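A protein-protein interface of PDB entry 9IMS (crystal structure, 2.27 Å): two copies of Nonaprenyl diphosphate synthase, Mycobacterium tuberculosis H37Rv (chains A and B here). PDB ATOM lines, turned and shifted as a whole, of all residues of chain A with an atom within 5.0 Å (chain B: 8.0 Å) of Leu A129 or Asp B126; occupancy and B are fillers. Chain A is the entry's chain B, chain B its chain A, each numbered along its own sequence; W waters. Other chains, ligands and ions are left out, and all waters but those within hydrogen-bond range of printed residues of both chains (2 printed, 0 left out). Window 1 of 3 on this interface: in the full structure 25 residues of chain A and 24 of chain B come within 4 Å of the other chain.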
ATOM      1  N   ILE A  89     -13.834  27.831  -5.112  1.00  0.00           N
ATOM      2  CA  ILE A  89     -14.748  27.329  -4.088  1.00  0.00           C
ATOM      3  C   ILE A  89     -16.081  26.961  -4.720  1.00  0.00           C
ATOM      4  O   ILE A  89     -16.604  25.860  -4.514  1.00  0.00           O
ATOM      5  CB  ILE A  89     -14.917  28.368  -2.960  1.00  0.00           C
ATOM      6  CG1 ILE A  89     -13.582  28.604  -2.245  1.00  0.00           C
ATOM      7  CG2 ILE A  89     -15.992  27.917  -1.960  1.00  0.00           C
ATOM      8  CD1 ILE A  89     -13.273  27.507  -1.203  1.00  0.00           C
ATOM      9  N   ALA A  92     -15.747  23.822  -6.753  1.00  0.00           N
ATOM     10  CA  ALA A  92     -15.605  22.625  -5.937  1.00  0.00           C
ATOM     11  C   ALA A  92     -16.962  22.137  -5.450  1.00  0.00           C
ATOM     12  O   ALA A  92     -17.219  20.925  -5.424  1.00  0.00           O
ATOM     13  CB  ALA A  92     -14.656  22.893  -4.766  1.00  0.00           C
ATOM     14  N   HIS A  96     -18.559  18.443  -5.848  1.00  0.00           N
ATOM     15  CA  HIS A  96     -19.039  17.655  -4.715  1.00  0.00           C
ATOM     16  C   HIS A  96     -20.547  17.438  -4.772  1.00  0.00           C
ATOM     17  O   HIS A  96     -21.037  16.407  -4.286  1.00  0.00           O
ATOM     18  CB  HIS A  96     -18.595  18.313  -3.401  1.00  0.00           C
ATOM     19  CG  HIS A  96     -17.157  18.045  -3.085  1.00  0.00           C
ATOM     20  ND1 HIS A  96     -16.543  18.470  -1.928  1.00  0.00           N
ATOM     21  CD2 HIS A  96     -16.210  17.377  -3.791  1.00  0.00           C
ATOM     22  CE1 HIS A  96     -15.282  18.071  -1.930  1.00  0.00           C
ATOM     23  NE2 HIS A  96     -15.053  17.411  -3.052  1.00  0.00           N
ATOM     24  N   GLY A 125     -13.203  18.134  -6.763  1.00  0.00           N
ATOM     25  CA  GLY A 125     -13.545  19.134  -5.759  1.00  0.00           C
ATOM     26  C   GLY A 125     -12.429  19.362  -4.748  1.00  0.00           C
ATOM     27  O   GLY A 125     -12.103  20.506  -4.414  1.00  0.00           O
ATOM     28  N   ASP A 126     -11.793  18.280  -4.280  1.00  0.00           N
ATOM     29  CA  ASP A 126     -10.713  18.459  -3.302  1.00  0.00           C
ATOM     30  C   ASP A 126      -9.510  19.156  -3.922  1.00  0.00           C
ATOM     31  O   ASP A 126      -8.757  19.848  -3.217  1.00  0.00           O
ATOM     32  CB  ASP A 126     -10.293  17.114  -2.700  1.00  0.00           C
ATOM     33  CG  ASP A 126     -11.309  16.580  -1.713  1.00  0.00           C
ATOM     34  OD1 ASP A 126     -12.300  17.300  -1.462  1.00  0.00           O
ATOM     35  OD2 ASP A 126     -11.117  15.459  -1.179  1.00  0.00           O
ATOM     36  N   TYR A 127      -9.320  18.992  -5.230  1.00  0.00           N
ATOM     37  CA  TYR A 127      -8.205  19.650  -5.902  1.00  0.00           C
ATOM     38  C   TYR A 127      -8.428  21.148  -5.965  1.00  0.00           C
ATOM     39  O   TYR A 127      -7.523  21.943  -5.666  1.00  0.00           O
ATOM     40  CB  TYR A 127      -8.034  19.080  -7.313  1.00  0.00           C
ATOM     41  CG  TYR A 127      -6.839  19.643  -8.061  1.00  0.00           C
ATOM     42  CD1 TYR A 127      -5.546  19.244  -7.742  1.00  0.00           C
ATOM     43  CD2 TYR A 127      -7.006  20.555  -9.094  1.00  0.00           C
ATOM     44  CE1 TYR A 127      -4.448  19.757  -8.430  1.00  0.00           C
ATOM     45  CE2 TYR A 127      -5.916  21.068  -9.787  1.00  0.00           C
ATOM     46  CZ  TYR A 127      -4.640  20.669  -9.444  1.00  0.00           C
ATOM     47  OH  TYR A 127      -3.555  21.168 -10.127  1.00  0.00           O
ATOM     48  N   LEU A 128      -9.626  21.548  -6.400  1.00  0.00           N
ATOM     49  CA  LEU A 128     -10.017  22.952  -6.378  1.00  0.00           C
ATOM     50  C   LEU A 128      -9.831  23.543  -4.984  1.00  0.00           C
ATOM     51  O   LEU A 128      -9.198  24.597  -4.816  1.00  0.00           O
ATOM     52  CB  LEU A 128     -11.474  23.074  -6.851  1.00  0.00           C
ATOM     53  CG  LEU A 128     -11.673  22.832  -8.368  1.00  0.00           C
ATOM     54  CD1 LEU A 128     -13.100  22.340  -8.730  1.00  0.00           C
ATOM     55  CD2 LEU A 128     -11.287  24.076  -9.183  1.00  0.00           C
ATOM     56  N   LEU A 129     -10.370  22.852  -3.968  1.00  0.00           N
ATOM     57  CA  LEU A 129     -10.225  23.271  -2.575  1.00  0.00           C
ATOM     58  C   LEU A 129      -8.756  23.466  -2.192  1.00  0.00           C
ATOM     59  O   LEU A 129      -8.369  24.522  -1.678  1.00  0.00           O
ATOM     60  CB  LEU A 129     -10.890  22.233  -1.660  1.00  0.00           C
ATOM     61  CG  LEU A 129     -12.421  22.177  -1.705  1.00  0.00           C
ATOM     62  CD1 LEU A 129     -12.971  21.205  -0.680  1.00  0.00           C
ATOM     63  CD2 LEU A 129     -12.976  23.545  -1.478  1.00  0.00           C
ATOM     64  N   ALA A 130      -7.922  22.457  -2.447  1.00  0.00           N
ATOM     65  CA  ALA A 130      -6.501  22.575  -2.116  1.00  0.00           C
ATOM     66  C   ALA A 130      -5.862  23.754  -2.839  1.00  0.00           C
ATOM     67  O   ALA A 130      -5.122  24.535  -2.233  1.00  0.00           O
ATOM     68  CB  ALA A 130      -5.766  21.275  -2.451  1.00  0.00           C
ATOM     69  N   THR A 131      -6.142  23.907  -4.134  1.00  0.00           N
ATOM     70  CA  THR A 131      -5.611  25.055  -4.862  1.00  0.00           C
ATOM     71  C   THR A 131      -6.127  26.367  -4.274  1.00  0.00           C
ATOM     72  O   THR A 131      -5.365  27.332  -4.115  1.00  0.00           O
ATOM     73  CB  THR A 131      -5.984  24.949  -6.342  1.00  0.00           C
ATOM     74  OG1 THR A 131      -5.783  23.598  -6.780  1.00  0.00           O
ATOM     75  CG2 THR A 131      -5.167  25.934  -7.202  1.00  0.00           C
ATOM     76  N   ALA A 132      -7.420  26.427  -3.943  1.00  0.00           N
ATOM     77  CA  ALA A 132      -7.931  27.628  -3.286  1.00  0.00           C
ATOM     78  C   ALA A 132      -7.198  27.895  -1.969  1.00  0.00           C
ATOM     79  O   ALA A 132      -6.891  29.053  -1.652  1.00  0.00           O
ATOM     80  CB  ALA A 132      -9.438  27.516  -3.063  1.00  0.00           C
ATOM     81  N   SER A 133      -6.887  26.837  -1.207  1.00  0.00           N
ATOM     82  CA  SER A 133      -6.140  26.989   0.049  1.00  0.00           C
ATOM     83  C   SER A 133      -4.807  27.679  -0.186  1.00  0.00           C
ATOM     84  O   SER A 133      -4.448  28.635   0.510  1.00  0.00           O
ATOM     85  CB  SER A 133      -5.877  25.624   0.698  1.00  0.00           C
ATOM     86  OG  SER A 133      -7.027  25.128   1.336  1.00  0.00           O
ATOM     87  N   PHE A 151     -17.027  28.894   3.321  1.00  0.00           N
ATOM     88  CA  PHE A 151     -17.188  27.515   2.884  1.00  0.00           C
ATOM     89  C   PHE A 151     -17.934  26.684   3.931  1.00  0.00           C
ATOM     90  O   PHE A 151     -18.810  25.878   3.589  1.00  0.00           O
ATOM     91  CB  PHE A 151     -15.810  26.925   2.587  1.00  0.00           C
ATOM     92  CG  PHE A 151     -15.850  25.553   1.957  1.00  0.00           C
ATOM     93  CD1 PHE A 151     -16.755  25.267   0.945  1.00  0.00           C
ATOM     94  CD2 PHE A 151     -14.966  24.552   2.369  1.00  0.00           C
ATOM     95  CE1 PHE A 151     -16.801  24.010   0.366  1.00  0.00           C
ATOM     96  CE2 PHE A 151     -14.994  23.284   1.785  1.00  0.00           C
ATOM     97  CZ  PHE A 151     -15.917  23.009   0.793  1.00  0.00           C
ATOM     98  N   VAL A 155     -21.429  24.918   3.253  1.00  0.00           N
ATOM     99  CA  VAL A 155     -21.654  23.498   3.505  1.00  0.00           C
ATOM    100  C   VAL A 155     -22.860  23.280   4.417  1.00  0.00           C
ATOM    101  O   VAL A 155     -23.687  22.398   4.157  1.00  0.00           O
ATOM    102  CB  VAL A 155     -20.379  22.863   4.083  1.00  0.00           C
ATOM    103  CG1 VAL A 155     -20.671  21.461   4.598  1.00  0.00           C
ATOM    104  CG2 VAL A 155     -19.314  22.808   2.989  1.00  0.00           C
ATOM    105  N   ASP B  46     -21.202  14.059  14.339  1.00  0.00           N
ATOM    106  CA  ASP B  46     -20.353  14.414  13.203  1.00  0.00           C
ATOM    107  C   ASP B  46     -18.897  14.005  13.418  1.00  0.00           C
ATOM    108  O   ASP B  46     -18.237  13.556  12.473  1.00  0.00           O
ATOM    109  CB  ASP B  46     -20.486  15.919  12.942  1.00  0.00           C
ATOM    110  CG  ASP B  46     -19.306  16.502  12.185  1.00  0.00           C
ATOM    111  OD1 ASP B  46     -19.180  16.259  10.964  1.00  0.00           O
ATOM    112  OD2 ASP B  46     -18.502  17.218  12.820  1.00  0.00           O
ATOM    113  N   MET B  88      -9.145  17.384  12.972  1.00  0.00           N
ATOM    114  CA  MET B  88     -10.304  17.602  12.110  1.00  0.00           C
ATOM    115  C   MET B  88      -9.955  17.261  10.665  1.00  0.00           C
ATOM    116  O   MET B  88     -10.744  16.625   9.953  1.00  0.00           O
ATOM    117  CB  MET B  88     -10.803  19.043  12.246  1.00  0.00           C
ATOM    118  CG  MET B  88     -11.856  19.209  13.363  1.00  0.00           C
ATOM    119  SD  MET B  88     -12.169  20.938  13.822  1.00  0.00           S
ATOM    120  CE  MET B  88     -12.051  21.494  12.200  1.00  0.00           C
ATOM    121  N   LEU B  91     -10.050  13.462  10.351  1.00  0.00           N
ATOM    122  CA  LEU B  91     -11.402  12.925  10.270  1.00  0.00           C
ATOM    123  C   LEU B  91     -12.010  13.175   8.897  1.00  0.00           C
ATOM    124  O   LEU B  91     -12.734  12.327   8.366  1.00  0.00           O
ATOM    125  CB  LEU B  91     -12.270  13.548  11.362  1.00  0.00           C
ATOM    126  CG  LEU B  91     -12.060  12.968  12.768  1.00  0.00           C
ATOM    127  CD1 LEU B  91     -12.575  13.930  13.786  1.00  0.00           C
ATOM    128  CD2 LEU B  91     -12.776  11.645  12.910  1.00  0.00           C
ATOM    129  N   ALA B  92     -11.720  14.334   8.306  1.00  0.00           N
ATOM    130  CA  ALA B  92     -12.270  14.644   6.995  1.00  0.00           C
ATOM    131  C   ALA B  92     -11.715  13.711   5.927  1.00  0.00           C
ATOM    132  O   ALA B  92     -12.462  13.249   5.055  1.00  0.00           O
ATOM    133  CB  ALA B  92     -11.994  16.109   6.641  1.00  0.00           C
ATOM    134  N   THR B  93     -10.406  13.423   5.968  1.00  0.00           N
ATOM    135  CA  THR B  93      -9.851  12.445   5.036  1.00  0.00           C
ATOM    136  C   THR B  93     -10.535  11.095   5.194  1.00  0.00           C
ATOM    137  O   THR B  93     -10.726  10.379   4.204  1.00  0.00           O
ATOM    138  CB  THR B  93      -8.341  12.283   5.232  1.00  0.00           C
ATOM    139  OG1 THR B  93      -8.087  11.717   6.525  1.00  0.00           O
ATOM    140  CG2 THR B  93      -7.616  13.612   5.117  1.00  0.00           C
ATOM    141  N   TYR B  95     -13.739  10.616   6.133  1.00  0.00           N
ATOM    142  CA  TYR B  95     -15.037  10.752   5.479  1.00  0.00           C
ATOM    143  C   TYR B  95     -14.902  10.630   3.958  1.00  0.00           C
ATOM    144  O   TYR B  95     -15.656   9.898   3.305  1.00  0.00           O
ATOM    145  CB  TYR B  95     -15.665  12.094   5.869  1.00  0.00           C
ATOM    146  CG  TYR B  95     -16.410  12.091   7.192  1.00  0.00           C
ATOM    147  CD1 TYR B  95     -17.733  11.677   7.259  1.00  0.00           C
ATOM    148  CD2 TYR B  95     -15.803  12.518   8.365  1.00  0.00           C
ATOM    149  CE1 TYR B  95     -18.431  11.680   8.456  1.00  0.00           C
ATOM    150  CE2 TYR B  95     -16.493  12.522   9.575  1.00  0.00           C
ATOM    151  CZ  TYR B  95     -17.808  12.100   9.610  1.00  0.00           C
ATOM    152  OH  TYR B  95     -18.515  12.088  10.790  1.00  0.00           O
ATOM    153  N   HIS B  96     -13.923  11.325   3.376  1.00  0.00           N
ATOM    154  CA  HIS B  96     -13.788  11.302   1.926  1.00  0.00           C
ATOM    155  C   HIS B  96     -13.309   9.945   1.443  1.00  0.00           C
ATOM    156  O   HIS B  96     -13.761   9.464   0.395  1.00  0.00           O
ATOM    157  CB  HIS B  96     -12.843  12.412   1.473  1.00  0.00           C
ATOM    158  CG  HIS B  96     -13.469  13.770   1.486  1.00  0.00           C
ATOM    159  ND1 HIS B  96     -12.922  14.850   0.825  1.00  0.00           N
ATOM    160  CD2 HIS B  96     -14.597  14.228   2.088  1.00  0.00           C
ATOM    161  CE1 HIS B  96     -13.681  15.915   1.022  1.00  0.00           C
ATOM    162  NE2 HIS B  96     -14.704  15.565   1.786  1.00  0.00           N
ATOM    163  N   ASN B 119     -23.249  11.550  -0.256  1.00  0.00           N
ATOM    164  CA  ASN B 119     -23.242  13.005  -0.399  1.00  0.00           C
ATOM    165  C   ASN B 119     -23.094  13.682   0.958  1.00  0.00           C
ATOM    166  O   ASN B 119     -22.334  14.650   1.106  1.00  0.00           O
ATOM    167  CB  ASN B 119     -24.521  13.467  -1.108  1.00  0.00           C
ATOM    168  CG  ASN B 119     -24.380  14.847  -1.747  1.00  0.00           C
ATOM    169  OD1 ASN B 119     -24.495  15.879  -1.072  1.00  0.00           O
ATOM    170  ND2 ASN B 119     -24.142  14.870  -3.062  1.00  0.00           N
ATOM    171  N   VAL B 120     -23.779  13.154   1.970  1.00  0.00           N
ATOM    172  CA  VAL B 120     -23.679  13.701   3.320  1.00  0.00           C
ATOM    173  C   VAL B 120     -22.287  13.480   3.907  1.00  0.00           C
ATOM    174  O   VAL B 120     -21.737  14.364   4.577  1.00  0.00           O
ATOM    175  CB  VAL B 120     -24.791  13.100   4.197  1.00  0.00           C
ATOM    176  CG1 VAL B 120     -24.382  13.049   5.656  1.00  0.00           C
ATOM    177  CG2 VAL B 120     -26.051  13.928   4.032  1.00  0.00           C
ATOM    178  N   ALA B 121     -21.685  12.311   3.664  1.00  0.00           N
ATOM    179  CA  ALA B 121     -20.347  12.065   4.194  1.00  0.00           C
ATOM    180  C   ALA B 121     -19.338  13.039   3.595  1.00  0.00           C
ATOM    181  O   ALA B 121     -18.408  13.495   4.282  1.00  0.00           O
ATOM    182  CB  ALA B 121     -19.931  10.620   3.923  1.00  0.00           C
ATOM    183  N   ILE B 122     -19.509  13.371   2.310  1.00  0.00           N
ATOM    184  CA  ILE B 122     -18.633  14.334   1.652  1.00  0.00           C
ATOM    185  C   ILE B 122     -18.820  15.720   2.255  1.00  0.00           C
ATOM    186  O   ILE B 122     -17.844  16.411   2.576  1.00  0.00           O
ATOM    187  CB  ILE B 122     -18.881  14.332   0.129  1.00  0.00           C
ATOM    188  CG1 ILE B 122     -18.299  13.070  -0.505  1.00  0.00           C
ATOM    189  CG2 ILE B 122     -18.263  15.558  -0.530  1.00  0.00           C
ATOM    190  CD1 ILE B 122     -16.953  12.663   0.068  1.00  0.00           C
ATOM    191  N   LEU B 123     -20.074  16.149   2.417  1.00  0.00           N
ATOM    192  CA  LEU B 123     -20.346  17.438   3.049  1.00  0.00           C
ATOM    193  C   LEU B 123     -19.730  17.509   4.440  1.00  0.00           C
ATOM    194  O   LEU B 123     -19.110  18.517   4.807  1.00  0.00           O
ATOM    195  CB  LEU B 123     -21.859  17.682   3.129  1.00  0.00           C
ATOM    196  CG  LEU B 123     -22.621  17.905   1.816  1.00  0.00           C
ATOM    197  CD1 LEU B 123     -24.094  18.170   2.085  1.00  0.00           C
ATOM    198  CD2 LEU B 123     -21.989  19.035   0.978  1.00  0.00           C
ATOM    199  N   ALA B 124     -19.914  16.454   5.239  1.00  0.00           N
ATOM    200  CA  ALA B 124     -19.337  16.422   6.583  1.00  0.00           C
ATOM    201  C   ALA B 124     -17.832  16.619   6.529  1.00  0.00           C
ATOM    202  O   ALA B 124     -17.270  17.415   7.292  1.00  0.00           O
ATOM    203  CB  ALA B 124     -19.674  15.101   7.275  1.00  0.00           C
ATOM    204  N   GLY B 125     -17.160  15.904   5.627  1.00  0.00           N
ATOM    205  CA  GLY B 125     -15.736  16.115   5.467  1.00  0.00           C
ATOM    206  C   GLY B 125     -15.418  17.535   5.053  1.00  0.00           C
ATOM    207  O   GLY B 125     -14.471  18.149   5.560  1.00  0.00           O
ATOM    208  N   ASP B 126     -16.218  18.090   4.144  1.00  0.00           N
ATOM    209  CA  ASP B 126     -15.965  19.457   3.721  1.00  0.00           C
ATOM    210  C   ASP B 126     -16.104  20.426   4.896  1.00  0.00           C
ATOM    211  O   ASP B 126     -15.274  21.323   5.072  1.00  0.00           O
ATOM    212  CB  ASP B 126     -16.899  19.814   2.562  1.00  0.00           C
ATOM    213  CG  ASP B 126     -16.455  19.190   1.244  1.00  0.00           C
ATOM    214  OD1 ASP B 126     -15.312  18.659   1.175  1.00  0.00           O
ATOM    215  OD2 ASP B 126     -17.245  19.234   0.272  1.00  0.00           O
ATOM    216  N   TYR B 127     -17.117  20.225   5.743  1.00  0.00           N
ATOM    217  CA  TYR B 127     -17.283  21.078   6.925  1.00  0.00           C
ATOM    218  C   TYR B 127     -16.094  20.955   7.876  1.00  0.00           C
ATOM    219  O   TYR B 127     -15.589  21.961   8.382  1.00  0.00           O
ATOM    220  CB  TYR B 127     -18.579  20.721   7.649  1.00  0.00           C
ATOM    221  CG  TYR B 127     -18.937  21.679   8.763  1.00  0.00           C
ATOM    222  CD1 TYR B 127     -19.368  22.975   8.487  1.00  0.00           C
ATOM    223  CD2 TYR B 127     -18.853  21.287  10.094  1.00  0.00           C
ATOM    224  CE1 TYR B 127     -19.702  23.852   9.504  1.00  0.00           C
ATOM    225  CE2 TYR B 127     -19.184  22.157  11.115  1.00  0.00           C
ATOM    226  CZ  TYR B 127     -19.606  23.434  10.815  1.00  0.00           C
ATOM    227  OH  TYR B 127     -19.927  24.295  11.828  1.00  0.00           O
ATOM    228  N   LEU B 128     -15.625  19.727   8.113  1.00  0.00           N
ATOM    229  CA  LEU B 128     -14.426  19.527   8.919  1.00  0.00           C
ATOM    230  C   LEU B 128     -13.233  20.261   8.323  1.00  0.00           C
ATOM    231  O   LEU B 128     -12.425  20.846   9.059  1.00  0.00           O
ATOM    232  CB  LEU B 128     -14.132  18.027   9.057  1.00  0.00           C
ATOM    233  CG  LEU B 128     -14.989  17.306  10.111  1.00  0.00           C
ATOM    234  CD1 LEU B 128     -15.094  15.807   9.830  1.00  0.00           C
ATOM    235  CD2 LEU B 128     -14.457  17.569  11.541  1.00  0.00           C
ATOM    236  N   LEU B 129     -13.109  20.256   6.985  1.00  0.00           N
ATOM    237  CA  LEU B 129     -11.988  20.953   6.360  1.00  0.00           C
ATOM    238  C   LEU B 129     -12.142  22.465   6.483  1.00  0.00           C
ATOM    239  O   LEU B 129     -11.160  23.183   6.707  1.00  0.00           O
ATOM    240  CB  LEU B 129     -11.856  20.539   4.892  1.00  0.00           C
ATOM    241  CG  LEU B 129     -11.368  19.103   4.716  1.00  0.00           C
ATOM    242  CD1 LEU B 129     -11.568  18.615   3.266  1.00  0.00           C
ATOM    243  CD2 LEU B 129      -9.917  18.975   5.168  1.00  0.00           C
ATOM    244  N   ALA B 130     -13.365  22.967   6.321  1.00  0.00           N
ATOM    245  CA  ALA B 130     -13.597  24.398   6.463  1.00  0.00           C
ATOM    246  C   ALA B 130     -13.294  24.853   7.886  1.00  0.00           C
ATOM    247  O   ALA B 130     -12.624  25.875   8.103  1.00  0.00           O
ATOM    248  CB  ALA B 130     -15.048  24.732   6.074  1.00  0.00           C
ATOM    249  N   THR B 131     -13.772  24.094   8.874  1.00  0.00           N
ATOM    250  CA  THR B 131     -13.536  24.476  10.263  1.00  0.00           C
ATOM    251  C   THR B 131     -12.054  24.393  10.615  1.00  0.00           C
ATOM    252  O   THR B 131     -11.540  25.238  11.359  1.00  0.00           O
ATOM    253  CB  THR B 131     -14.392  23.611  11.192  1.00  0.00           C
ATOM    254  OG1 THR B 131     -15.747  23.633  10.738  1.00  0.00           O
ATOM    255  CG2 THR B 131     -14.352  24.129  12.637  1.00  0.00           C
ATOM    256  N   ALA B 132     -11.331  23.409  10.064  1.00  0.00           N
ATOM    257  CA  ALA B 132      -9.897  23.341  10.349  1.00  0.00           C
ATOM    258  C   ALA B 132      -9.180  24.552   9.776  1.00  0.00           C
ATOM    259  O   ALA B 132      -8.299  25.128  10.429  1.00  0.00           O
ATOM    260  CB  ALA B 132      -9.291  22.055   9.793  1.00  0.00           C
ATOM    261  N   SER B 133      -9.580  24.976   8.574  1.00  0.00           N
ATOM    262  CA  SER B 133      -8.938  26.128   7.952  1.00  0.00           C
ATOM    263  C   SER B 133      -9.235  27.399   8.732  1.00  0.00           C
ATOM    264  O   SER B 133      -8.338  28.229   8.932  1.00  0.00           O
ATOM    265  CB  SER B 133      -9.390  26.268   6.499  1.00  0.00           C
ATOM    266  OG  SER B 133      -9.351  25.017   5.849  1.00  0.00           O
ATOM    267  N   ALA B 148      -1.921  24.606   4.241  1.00  0.00           N
ATOM    268  CA  ALA B 148      -2.213  24.603   2.807  1.00  0.00           C
ATOM    269  C   ALA B 148      -1.297  23.632   2.070  1.00  0.00           C
ATOM    270  O   ALA B 148      -1.742  22.877   1.195  1.00  0.00           O
ATOM    271  CB  ALA B 148      -2.086  26.016   2.221  1.00  0.00           C
ATOM    272  N   PHE B 151      -2.587  20.124   2.770  1.00  0.00           N
ATOM    273  CA  PHE B 151      -3.698  19.817   1.884  1.00  0.00           C
ATOM    274  C   PHE B 151      -3.192  19.391   0.508  1.00  0.00           C
ATOM    275  O   PHE B 151      -3.693  18.429  -0.078  1.00  0.00           O
ATOM    276  CB  PHE B 151      -4.625  21.028   1.742  1.00  0.00           C
ATOM    277  CG  PHE B 151      -5.451  21.339   2.970  1.00  0.00           C
ATOM    278  CD1 PHE B 151      -5.877  20.335   3.826  1.00  0.00           C
ATOM    279  CD2 PHE B 151      -5.814  22.653   3.254  1.00  0.00           C
ATOM    280  CE1 PHE B 151      -6.661  20.637   4.945  1.00  0.00           C
ATOM    281  CE2 PHE B 151      -6.596  22.966   4.396  1.00  0.00           C
ATOM    282  CZ  PHE B 151      -7.015  21.951   5.233  1.00  0.00           C
ATOM    283  N   ALA B 152      -2.194  20.101  -0.020  1.00  0.00           N
ATOM    284  CA  ALA B 152      -1.656  19.745  -1.331  1.00  0.00           C
ATOM    285  C   ALA B 152      -1.108  18.324  -1.332  1.00  0.00           C
ATOM    286  O   ALA B 152      -1.362  17.557  -2.264  1.00  0.00           O
ATOM    287  CB  ALA B 152      -0.575  20.743  -1.748  1.00  0.00           C
ATOM    288  N   VAL B 155      -4.122  15.732  -1.276  1.00  0.00           N
ATOM    289  CA  VAL B 155      -4.759  15.536  -2.571  1.00  0.00           C
ATOM    290  C   VAL B 155      -3.807  14.826  -3.530  1.00  0.00           C
ATOM    291  O   VAL B 155      -4.225  13.988  -4.339  1.00  0.00           O
ATOM    292  CB  VAL B 155      -5.239  16.890  -3.128  1.00  0.00           C
ATOM    293  CG1 VAL B 155      -5.873  16.717  -4.505  1.00  0.00           C
ATOM    294  CG2 VAL B 155      -6.235  17.518  -2.167  1.00  0.00           C
HETATM  295  O   HOH W   1      -2.547  23.508  -1.127  1.00  0.00           O
HETATM  296  O   HOH W   2     -21.281  16.073  -1.506  1.00  0.00           O
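His A96 touches its own counterpart, His B96.
Asp A126 touches Val B155, and with the chains exchanged Val A155 touches Asp B126.
Ala A130 touches Val B155, but with the chains exchanged Val A155 does not touch Ala B130 (5.6 Å).
Phe A151 touches Asp B126, but with the chains exchanged Asp A126 does not touch Phe B151 (6.1 Å).
Positions printed for both chains: 92, 96, 125, 126, 127, 128, 129, 130, 131, 132, 133, 151 and 155.
Of the 16 pairs that touch across the chains among the printed residues, 7 have their exchanged pair printed and touching as well.
Of chain A, only His A96 (2.4 Å), Leu A129 (3.9 Å), Phe A151 (3.8 Å) and Val A155 (3.9 Å) come within 4 Å of Asp B126.
Of chain B, only Val B155 comes within 4 Å of Ala A130.
Printed residues of chain B within 4 Å of Val A155: Leu B123 (3.3 Å), Asp B126 (3.9 Å) and Tyr B127 (3.8 Å).
Of the printed residues of chain A, Phe B151 touches Ser A133.
Of the printed residues of chain B, His A96 touches His B96, Asn B119, Ile B122 and Asp B126.
Of the printed residues of chain A, Tyr B127 touches Val A155.
Of the printed residues of chain B, Ser A133 touches Ala B148 (3.9 Å) and Phe B151 (3.4 Å).
Thr B93 touches none of the printed residues of chain A.
The nearest residue of chain B that does not touch Leu A129 is Leu B129 (4.9 Å).
The nearest residue of chain A that does not touch Asp B126 is Asp A126 (4.2 Å).
The nearest printed residue of chain A that does not touch Leu B123 is His A96 (5.6 Å).
Printed residues of chain B that touch a printed residue of chain A: His B96, Asn B119, Ile B122, Leu B123, Asp B126, Tyr B127, Ala B130, Ala B148, Phe B151 and Val B155.
Printed residues of chain A that touch a printed residue of chain B: His A96, Asp A126, Tyr A127, Leu A129, Ala A130, Ser A133, Phe A151 and Val A155.
Among the printed residues, 16 pairs touch across the chains.
Among the printed residues, no Asp or Glu carboxylate lies within 4 Å of a Lys or Arg side-chain nitrogen of the other chain.
Among the printed residues, pairs that only touch across the chains: Val A155 with Leu B123, Ser A133 with Phe B151, Asp A126 with Val B155, His A96 with Ile B122, His A96 with Asn B119, Phe A151 with Ala B130, Val A155 with Tyr B127, Phe A151 with Asp B126, Ala A130 with Val B155, Val A155 with Asp B126, Ser A133 with Ala B148, Leu A129 with Asp B126, His A96 with His B96 and Tyr A127 with Val B155.
The side-chain hydroxyl (OG1) of Thr B131 is in hydrogen-bond range of the backbone carbonyl oxygen (O) of Tyr B127 (2.9 Å).
The side-chain carboxylate of Asp A126 sits close to a ring nitrogen (NE2) of His A96 (3.2 Å).
A ring nitrogen (NE2) of His B96 sits close to the side-chain carboxylate of Asp B126, 3.2 Å away.
O of Leu A129 is in hydrogen-bond range of OG of Ser A133 (3.4 Å).
The side-chain hydroxyl (OG1) of Thr A131 lies within hydrogen-bond range of the backbone carbonyl oxygen (O) of Tyr A127 (2.6 Å).
A ring nitrogen (NE2) of His B96 lies within hydrogen-bond range of the backbone carbonyl oxygen (O) of Ile B122 (3.3 Å).
ND1 of His B96 is in hydrogen-bond range of OD2 of Asp A126 (2.8 Å).
The side-chain carboxylate (OD2) of Asp B126 lies within hydrogen-bond range of a ring nitrogen (ND1) of His A96.
Water W1 bridges O of Ala B148 and O of Ala A130.
Water W2 lies within hydrogen-bond range of the backbone carbonyl oxygen of His A96 and the backbone carbonyl oxygen of Asn B119.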
